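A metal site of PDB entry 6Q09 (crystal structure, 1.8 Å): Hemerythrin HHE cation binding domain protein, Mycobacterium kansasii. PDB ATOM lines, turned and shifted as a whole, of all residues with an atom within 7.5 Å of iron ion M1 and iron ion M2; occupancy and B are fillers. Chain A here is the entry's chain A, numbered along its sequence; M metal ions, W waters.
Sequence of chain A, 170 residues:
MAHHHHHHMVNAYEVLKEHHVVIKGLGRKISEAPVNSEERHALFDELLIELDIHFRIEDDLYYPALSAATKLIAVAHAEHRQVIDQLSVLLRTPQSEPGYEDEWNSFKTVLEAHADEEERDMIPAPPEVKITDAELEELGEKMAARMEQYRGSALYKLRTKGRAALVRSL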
ATOM      1  N   LEU A  16      -7.760 -19.846 -16.305  1.00  0.00           N
ATOM      2  CA  LEU A  16      -8.000 -19.396 -14.931  1.00  0.00           C
ATOM      3  C   LEU A  16      -6.780 -18.672 -14.382  1.00  0.00           C
ATOM      4  O   LEU A  16      -6.915 -17.653 -13.689  1.00  0.00           O
ATOM      5  CB  LEU A  16      -8.336 -20.571 -14.023  1.00  0.00           C
ATOM      6  CG  LEU A  16      -9.706 -21.150 -14.316  1.00  0.00           C
ATOM      7  CD1 LEU A  16      -9.882 -22.429 -13.538  1.00  0.00           C
ATOM      8  CD2 LEU A  16     -10.795 -20.148 -13.958  1.00  0.00           C
ATOM      9  N   LYS A  17      -5.581 -19.175 -14.670  1.00  0.00           N
ATOM     10  CA  LYS A  17      -4.398 -18.505 -14.136  1.00  0.00           C
ATOM     11  C   LYS A  17      -4.238 -17.107 -14.727  1.00  0.00           C
ATOM     12  O   LYS A  17      -3.934 -16.148 -14.005  1.00  0.00           O
ATOM     13  CB  LYS A  17      -3.161 -19.343 -14.387  1.00  0.00           C
ATOM     14  CG  LYS A  17      -3.093 -20.607 -13.560  1.00  0.00           C
ATOM     15  CD  LYS A  17      -1.922 -21.435 -14.042  1.00  0.00           C
ATOM     16  CE  LYS A  17      -0.974 -21.755 -12.928  1.00  0.00           C
ATOM     17  NZ  LYS A  17       0.265 -22.347 -13.508  1.00  0.00           N
ATOM     18  N   HIS A  19      -6.636 -15.253 -15.902  1.00  0.00           N
ATOM     19  CA  HIS A  19      -7.679 -14.387 -15.368  1.00  0.00           C
ATOM     20  C   HIS A  19      -7.382 -14.000 -13.929  1.00  0.00           C
ATOM     21  O   HIS A  19      -7.745 -12.892 -13.503  1.00  0.00           O
ATOM     22  CB  HIS A  19      -9.053 -15.047 -15.463  1.00  0.00           C
ATOM     23  CG  HIS A  19     -10.169 -14.058 -15.443  1.00  0.00           C
ATOM     24  ND1 HIS A  19     -11.290 -14.211 -14.664  1.00  0.00           N
ATOM     25  CD2 HIS A  19     -10.290 -12.843 -16.032  1.00  0.00           C
ATOM     26  CE1 HIS A  19     -12.070 -13.151 -14.796  1.00  0.00           C
ATOM     27  NE2 HIS A  19     -11.498 -12.314 -15.636  1.00  0.00           N
ATOM     28  N   HIS A  20      -6.756 -14.892 -13.160  1.00  0.00           N
ATOM     29  CA  HIS A  20      -6.295 -14.525 -11.830  1.00  0.00           C
ATOM     30  C   HIS A  20      -5.326 -13.352 -11.882  1.00  0.00           C
ATOM     31  O   HIS A  20      -5.394 -12.441 -11.041  1.00  0.00           O
ATOM     32  CB  HIS A  20      -5.621 -15.708 -11.142  1.00  0.00           C
ATOM     33  CG  HIS A  20      -6.572 -16.721 -10.580  1.00  0.00           C
ATOM     34  ND1 HIS A  20      -6.228 -18.035 -10.351  1.00  0.00           N
ATOM     35  CD2 HIS A  20      -7.873 -16.609 -10.190  1.00  0.00           C
ATOM     36  CE1 HIS A  20      -7.260 -18.686  -9.854  1.00  0.00           C
ATOM     37  NE2 HIS A  20      -8.268 -17.845  -9.751  1.00  0.00           N
ATOM     38  N   ILE A  23      -7.318 -10.254 -12.254  1.00  0.00           N
ATOM     39  CA  ILE A  23      -8.042  -9.848 -11.043  1.00  0.00           C
ATOM     40  C   ILE A  23      -7.064  -9.266 -10.016  1.00  0.00           C
ATOM     41  O   ILE A  23      -7.326  -8.231  -9.373  1.00  0.00           O
ATOM     42  CB  ILE A  23      -8.811 -11.052 -10.469  1.00  0.00           C
ATOM     43  CG1 ILE A  23     -10.010 -11.347 -11.378  1.00  0.00           C
ATOM     44  CG2 ILE A  23      -9.231 -10.787  -8.992  1.00  0.00           C
ATOM     45  CD1 ILE A  23     -10.621 -12.727 -11.127  1.00  0.00           C
ATOM     46  N   HIS A  54     -15.596 -14.598 -13.302  1.00  0.00           N
ATOM     47  CA  HIS A  54     -14.663 -15.608 -12.827  1.00  0.00           C
ATOM     48  C   HIS A  54     -15.358 -16.694 -12.026  1.00  0.00           C
ATOM     49  O   HIS A  54     -15.195 -17.898 -12.289  1.00  0.00           O
ATOM     50  CB  HIS A  54     -13.562 -14.953 -11.966  1.00  0.00           C
ATOM     51  CG  HIS A  54     -12.415 -15.874 -11.647  1.00  0.00           C
ATOM     52  ND1 HIS A  54     -11.379 -16.101 -12.527  1.00  0.00           N
ATOM     53  CD2 HIS A  54     -12.131 -16.598 -10.538  1.00  0.00           C
ATOM     54  CE1 HIS A  54     -10.512 -16.929 -11.973  1.00  0.00           C
ATOM     55  NE2 HIS A  54     -10.955 -17.260 -10.779  1.00  0.00           N
ATOM     56  N   PHE A  55     -16.153 -16.291 -11.046  1.00  0.00           N
ATOM     57  CA  PHE A  55     -16.805 -17.311 -10.230  1.00  0.00           C
ATOM     58  C   PHE A  55     -17.796 -18.093 -11.061  1.00  0.00           C
ATOM     59  O   PHE A  55     -18.014 -19.288 -10.799  1.00  0.00           O
ATOM     60  CB  PHE A  55     -17.502 -16.677  -9.031  1.00  0.00           C
ATOM     61  CG  PHE A  55     -16.541 -16.247  -7.934  1.00  0.00           C
ATOM     62  CD1 PHE A  55     -15.188 -16.569  -8.018  1.00  0.00           C
ATOM     63  CD2 PHE A  55     -17.002 -15.562  -6.827  1.00  0.00           C
ATOM     64  CE1 PHE A  55     -14.276 -16.177  -7.008  1.00  0.00           C
ATOM     65  CE2 PHE A  55     -16.111 -15.169  -5.831  1.00  0.00           C
ATOM     66  CZ  PHE A  55     -14.743 -15.482  -5.920  1.00  0.00           C
ATOM     67  N   ILE A  57     -17.586 -18.856 -14.419  1.00  0.00           N
ATOM     68  CA  ILE A  57     -16.972 -19.899 -15.229  1.00  0.00           C
ATOM     69  C   ILE A  57     -16.444 -21.019 -14.336  1.00  0.00           C
ATOM     70  O   ILE A  57     -16.489 -22.190 -14.750  1.00  0.00           O
ATOM     71  CB  ILE A  57     -15.895 -19.347 -16.185  1.00  0.00           C
ATOM     72  CG1 ILE A  57     -14.656 -18.862 -15.440  1.00  0.00           C
ATOM     73  CG2 ILE A  57     -16.473 -18.233 -17.051  1.00  0.00           C
ATOM     74  CD1 ILE A  57     -13.414 -19.141 -16.238  1.00  0.00           C
ATOM     75  N   GLU A  58     -15.984 -20.720 -13.117  1.00  0.00           N
ATOM     76  CA  GLU A  58     -15.599 -21.788 -12.186  1.00  0.00           C
ATOM     77  C   GLU A  58     -16.804 -22.655 -11.793  1.00  0.00           C
ATOM     78  O   GLU A  58     -16.761 -23.888 -11.899  1.00  0.00           O
ATOM     79  CB  GLU A  58     -14.869 -21.198 -10.950  1.00  0.00           C
ATOM     80  CG  GLU A  58     -13.491 -20.708 -11.363  1.00  0.00           C
ATOM     81  CD  GLU A  58     -12.713 -20.214 -10.180  1.00  0.00           C
ATOM     82  OE1 GLU A  58     -13.328 -20.114  -9.103  1.00  0.00           O
ATOM     83  OE2 GLU A  58     -11.523 -19.968 -10.376  1.00  0.00           O
ATOM     84  N   ASP A  59     -17.929 -22.023 -11.389  1.00  0.00           N
ATOM     85  CA  ASP A  59     -19.059 -22.827 -10.926  1.00  0.00           C
ATOM     86  C   ASP A  59     -19.685 -23.591 -12.065  1.00  0.00           C
ATOM     87  O   ASP A  59     -20.214 -24.692 -11.861  1.00  0.00           O
ATOM     88  CB  ASP A  59     -20.150 -21.958 -10.308  1.00  0.00           C
ATOM     89  CG  ASP A  59     -19.728 -21.302  -9.023  1.00  0.00           C
ATOM     90  OD1 ASP A  59     -18.750 -21.772  -8.411  1.00  0.00           O
ATOM     91  OD2 ASP A  59     -20.389 -20.316  -8.647  1.00  0.00           O
ATOM     92  N   TYR A  62     -15.703 -25.183 -14.742  1.00  0.00           N
ATOM     93  CA  TYR A  62     -14.451 -25.753 -14.248  1.00  0.00           C
ATOM     94  C   TYR A  62     -14.692 -26.742 -13.111  1.00  0.00           C
ATOM     95  O   TYR A  62     -14.220 -27.880 -13.162  1.00  0.00           O
ATOM     96  CB  TYR A  62     -13.498 -24.654 -13.784  1.00  0.00           C
ATOM     97  CG  TYR A  62     -12.104 -25.199 -13.469  1.00  0.00           C
ATOM     98  CD1 TYR A  62     -11.302 -25.723 -14.467  1.00  0.00           C
ATOM     99  CD2 TYR A  62     -11.595 -25.166 -12.148  1.00  0.00           C
ATOM    100  CE1 TYR A  62     -10.045 -26.223 -14.200  1.00  0.00           C
ATOM    101  CE2 TYR A  62     -10.304 -25.641 -11.869  1.00  0.00           C
ATOM    102  CZ  TYR A  62      -9.544 -26.163 -12.893  1.00  0.00           C
ATOM    103  OH  TYR A  62      -8.298 -26.667 -12.661  1.00  0.00           O
ATOM    104  N   TYR A  63     -15.400 -26.313 -12.075  1.00  0.00           N
ATOM    105  CA  TYR A  63     -15.620 -27.211 -10.956  1.00  0.00           C
ATOM    106  C   TYR A  63     -16.421 -28.446 -11.357  1.00  0.00           C
ATOM    107  O   TYR A  63     -16.084 -29.541 -10.886  1.00  0.00           O
ATOM    108  CB  TYR A  63     -16.309 -26.488  -9.793  1.00  0.00           C
ATOM    109  CG  TYR A  63     -15.471 -25.426  -9.118  1.00  0.00           C
ATOM    110  CD1 TYR A  63     -14.100 -25.400  -9.243  1.00  0.00           C
ATOM    111  CD2 TYR A  63     -16.078 -24.435  -8.339  1.00  0.00           C
ATOM    112  CE1 TYR A  63     -13.324 -24.405  -8.613  1.00  0.00           C
ATOM    113  CE2 TYR A  63     -15.343 -23.468  -7.709  1.00  0.00           C
ATOM    114  CZ  TYR A  63     -13.968 -23.460  -7.855  1.00  0.00           C
ATOM    115  OH  TYR A  63     -13.262 -22.487  -7.217  1.00  0.00           O
ATOM    116  N   ALA A  76     -14.008 -25.250  -2.164  1.00  0.00           N
ATOM    117  CA  ALA A  76     -13.954 -24.143  -3.120  1.00  0.00           C
ATOM    118  C   ALA A  76     -15.271 -23.378  -3.182  1.00  0.00           C
ATOM    119  O   ALA A  76     -15.284 -22.144  -3.231  1.00  0.00           O
ATOM    120  CB  ALA A  76     -13.564 -24.670  -4.501  1.00  0.00           C
ATOM    121  N   HIS A  77     -16.410 -24.094  -3.186  1.00  0.00           N
ATOM    122  CA  HIS A  77     -17.694 -23.399  -3.101  1.00  0.00           C
ATOM    123  C   HIS A  77     -17.814 -22.611  -1.800  1.00  0.00           C
ATOM    124  O   HIS A  77     -18.392 -21.519  -1.782  1.00  0.00           O
ATOM    125  CB  HIS A  77     -18.839 -24.408  -3.231  1.00  0.00           C
ATOM    126  CG  HIS A  77     -19.070 -24.831  -4.639  1.00  0.00           C
ATOM    127  ND1 HIS A  77     -19.254 -26.137  -5.004  1.00  0.00           N
ATOM    128  CD2 HIS A  77     -19.167 -24.101  -5.783  1.00  0.00           C
ATOM    129  CE1 HIS A  77     -19.426 -26.208  -6.311  1.00  0.00           C
ATOM    130  NE2 HIS A  77     -19.388 -24.990  -6.814  1.00  0.00           N
ATOM    131  N   GLU A  79     -15.317 -21.290  -0.129  1.00  0.00           N
ATOM    132  CA  GLU A  79     -14.480 -20.107  -0.255  1.00  0.00           C
ATOM    133  C   GLU A  79     -15.115 -19.047  -1.150  1.00  0.00           C
ATOM    134  O   GLU A  79     -14.942 -17.850  -0.898  1.00  0.00           O
ATOM    135  CB  GLU A  79     -13.108 -20.493  -0.786  1.00  0.00           C
ATOM    136  CG  GLU A  79     -12.464 -21.544   0.074  1.00  0.00           C
ATOM    137  CD  GLU A  79     -10.976 -21.388   0.173  1.00  0.00           C
ATOM    138  OE1 GLU A  79     -10.359 -20.922  -0.812  1.00  0.00           O
ATOM    139  OE2 GLU A  79     -10.449 -21.687   1.257  1.00  0.00           O
ATOM    140  N   HIS A  80     -15.874 -19.456  -2.189  1.00  0.00           N
ATOM    141  CA  HIS A  80     -16.590 -18.454  -2.962  1.00  0.00           C
ATOM    142  C   HIS A  80     -17.584 -17.715  -2.071  1.00  0.00           C
ATOM    143  O   HIS A  80     -17.741 -16.488  -2.181  1.00  0.00           O
ATOM    144  CB  HIS A  80     -17.296 -19.076  -4.176  1.00  0.00           C
ATOM    145  CG  HIS A  80     -16.358 -19.397  -5.299  1.00  0.00           C
ATOM    146  ND1 HIS A  80     -16.796 -19.755  -6.558  1.00  0.00           N
ATOM    147  CD2 HIS A  80     -15.008 -19.418  -5.339  1.00  0.00           C
ATOM    148  CE1 HIS A  80     -15.739 -19.978  -7.327  1.00  0.00           C
ATOM    149  NE2 HIS A  80     -14.647 -19.786  -6.607  1.00  0.00           N
ATOM    150  N   VAL A  83     -15.751 -15.009  -0.035  1.00  0.00           N
ATOM    151  CA  VAL A  83     -15.517 -13.805  -0.826  1.00  0.00           C
ATOM    152  C   VAL A  83     -16.804 -13.005  -0.987  1.00  0.00           C
ATOM    153  O   VAL A  83     -16.814 -11.784  -0.819  1.00  0.00           O
ATOM    154  CB  VAL A  83     -14.909 -14.181  -2.181  1.00  0.00           C
ATOM    155  CG1 VAL A  83     -14.765 -12.955  -3.049  1.00  0.00           C
ATOM    156  CG2 VAL A  83     -13.577 -14.883  -1.984  1.00  0.00           C
ATOM    157  N   LEU A 111     -10.094 -12.522  -0.800  1.00  0.00           N
ATOM    158  CA  LEU A 111     -10.125 -12.865  -2.219  1.00  0.00           C
ATOM    159  C   LEU A 111      -8.799 -13.482  -2.663  1.00  0.00           C
ATOM    160  O   LEU A 111      -8.770 -14.536  -3.314  1.00  0.00           O
ATOM    161  CB  LEU A 111     -10.456 -11.614  -3.046  1.00  0.00           C
ATOM    162  CG  LEU A 111     -10.382 -11.731  -4.576  1.00  0.00           C
ATOM    163  CD1 LEU A 111     -11.380 -12.774  -5.094  1.00  0.00           C
ATOM    164  CD2 LEU A 111     -10.627 -10.384  -5.219  1.00  0.00           C
ATOM    165  N   HIS A 114      -8.272 -17.123  -1.287  1.00  0.00           N
ATOM    166  CA  HIS A 114      -9.011 -18.083  -2.108  1.00  0.00           C
ATOM    167  C   HIS A 114      -8.255 -18.407  -3.394  1.00  0.00           C
ATOM    168  O   HIS A 114      -8.015 -19.570  -3.708  1.00  0.00           O
ATOM    169  CB  HIS A 114     -10.404 -17.555  -2.428  1.00  0.00           C
ATOM    170  CG  HIS A 114     -10.994 -18.207  -3.638  1.00  0.00           C
ATOM    171  ND1 HIS A 114     -11.314 -19.551  -3.683  1.00  0.00           N
ATOM    172  CD2 HIS A 114     -11.261 -17.715  -4.865  1.00  0.00           C
ATOM    173  CE1 HIS A 114     -11.791 -19.841  -4.876  1.00  0.00           C
ATOM    174  NE2 HIS A 114     -11.770 -18.746  -5.613  1.00  0.00           N
ATOM    175  N   ALA A 115      -7.872 -17.369  -4.143  1.00  0.00           N
ATOM    176  CA  ALA A 115      -7.208 -17.620  -5.429  1.00  0.00           C
ATOM    177  C   ALA A 115      -5.900 -18.359  -5.260  1.00  0.00           C
ATOM    178  O   ALA A 115      -5.493 -19.146  -6.129  1.00  0.00           O
ATOM    179  CB  ALA A 115      -6.988 -16.305  -6.183  1.00  0.00           C
ATOM    180  N   ASP A 116      -5.212 -18.138  -4.146  1.00  0.00           N
ATOM    181  CA  ASP A 116      -3.986 -18.882  -3.900  1.00  0.00           C
ATOM    182  C   ASP A 116      -4.288 -20.318  -3.484  1.00  0.00           C
ATOM    183  O   ASP A 116      -3.601 -21.256  -3.915  1.00  0.00           O
ATOM    184  CB  ASP A 116      -3.128 -18.175  -2.857  1.00  0.00           C
ATOM    185  CG  ASP A 116      -2.515 -16.872  -3.369  1.00  0.00           C
ATOM    186  OD1 ASP A 116      -2.394 -16.707  -4.600  1.00  0.00           O
ATOM    187  OD2 ASP A 116      -2.143 -16.016  -2.540  1.00  0.00           O
ATOM    188  N   GLU A 118      -6.836 -21.925  -4.408  1.00  0.00           N
ATOM    189  CA  GLU A 118      -7.249 -22.545  -5.666  1.00  0.00           C
ATOM    190  C   GLU A 118      -6.043 -23.032  -6.460  1.00  0.00           C
ATOM    191  O   GLU A 118      -5.995 -24.185  -6.904  1.00  0.00           O
ATOM    192  CB  GLU A 118      -8.027 -21.530  -6.468  1.00  0.00           C
ATOM    193  CG  GLU A 118      -8.870 -22.068  -7.559  1.00  0.00           C
ATOM    194  CD  GLU A 118      -9.875 -21.014  -7.979  1.00  0.00           C
ATOM    195  OE1 GLU A 118      -9.452 -20.096  -8.714  1.00  0.00           O
ATOM    196  OE2 GLU A 118     -11.035 -21.080  -7.512  1.00  0.00           O
ATOM    197  N   GLU A 119      -5.028 -22.176  -6.639  1.00  0.00           N
ATOM    198  CA  GLU A 119      -3.832 -22.615  -7.345  1.00  0.00           C
ATOM    199  C   GLU A 119      -2.998 -23.616  -6.546  1.00  0.00           C
ATOM    200  O   GLU A 119      -2.047 -24.191  -7.089  1.00  0.00           O
ATOM    201  CB  GLU A 119      -2.987 -21.413  -7.757  1.00  0.00           C
ATOM    202  CG  GLU A 119      -3.451 -20.821  -9.088  1.00  0.00           C
ATOM    203  CD  GLU A 119      -2.977 -19.424  -9.326  1.00  0.00           C
ATOM    204  OE1 GLU A 119      -1.996 -19.004  -8.674  1.00  0.00           O
ATOM    205  OE2 GLU A 119      -3.570 -18.739 -10.186  1.00  0.00           O
ATOM    206  N   ILE A 123      -5.645 -26.305  -9.271  1.00  0.00           N
ATOM    207  CA  ILE A 123      -4.969 -26.110 -10.561  1.00  0.00           C
ATOM    208  C   ILE A 123      -3.554 -26.667 -10.446  1.00  0.00           C
ATOM    209  O   ILE A 123      -2.729 -26.094  -9.713  1.00  0.00           O
ATOM    210  CB  ILE A 123      -4.961 -24.633 -10.989  1.00  0.00           C
ATOM    211  CG1 ILE A 123      -6.399 -24.079 -11.076  1.00  0.00           C
ATOM    212  CG2 ILE A 123      -4.230 -24.472 -12.306  1.00  0.00           C
ATOM    213  CD1 ILE A 123      -6.484 -22.565 -11.316  1.00  0.00           C
HETATM  214 FE    FE M   1     -10.306 -18.498  -9.461  1.00  0.00          FE
HETATM  215 FE    FE M   2     -12.389 -19.654  -7.337  1.00  0.00          FE
HETATM  216  O   HOH W   1     -10.939 -17.765  -8.057  1.00  0.00           O
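A ring nitrogen (NE2) of His 80 lies close to the side-chain hydroxyl of Tyr 63 (3.1 Å).
The backbone carbonyl oxygen of Glu 58 lies within hydrogen-bond range of the backbone NH of Tyr 63 (2.8 Å).
A ring nitrogen (ND1) of His 114 is in hydrogen-bond range of the side-chain carboxylate of Glu 79, at 3.3 Å.
OE2 of Glu 118 lies close to OH of Tyr 63, 2.7 Å away.
ND1 of His 19 lies within hydrogen-bond range of ND1 of His 54.
The backbone carbonyl oxygen of Glu 118 sits at hydrogen-bond distance from the backbone NH of Ile 123, 3.2 Å away.
The side-chain carboxylate of Asp 59 lies within hydrogen-bond range of a ring nitrogen (ND1) of His 80.
OE2 of Glu 119 lies within hydrogen-bond range of ND1 of His 20 (2.8 Å).
CE1 of Phe 55 touches iron ion M2, at 3.97 Å.
Tyr 63 touches iron ion M2.
Within 4 Å of iron ion M2: Phe 55, Glu 58, Tyr 63, His 80, His 114 and Glu 118.
The nearest printed residue that does not touch iron ion M2 is His 54 (4.4 Å).
Water W1 binds iron ion M1, 1.7 Å away.
A ring nitrogen (NE2) of His 54 is bound to iron ion M1 (1.9 Å).
OE1 of Glu 118 binds iron ion M1.
OE2 of Glu 58 is bound to iron ion M1, at 2.1 Å.
A ring nitrogen (NE2) of His 20 binds iron ion M1 (2.2 Å).
Iron ion M2 is bound by the side-chain carboxylate (OE2) of Glu 118, at 2.0 Å.
NE2 of His 114 is bound to iron ion M2 (2.0 Å).
OE1 of Glu 58 binds iron ion M2 (2.1 Å).
Iron ion M2 is bound by NE2 of His 80, 2.4 Å away.
Water W1 binds iron ion M2.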
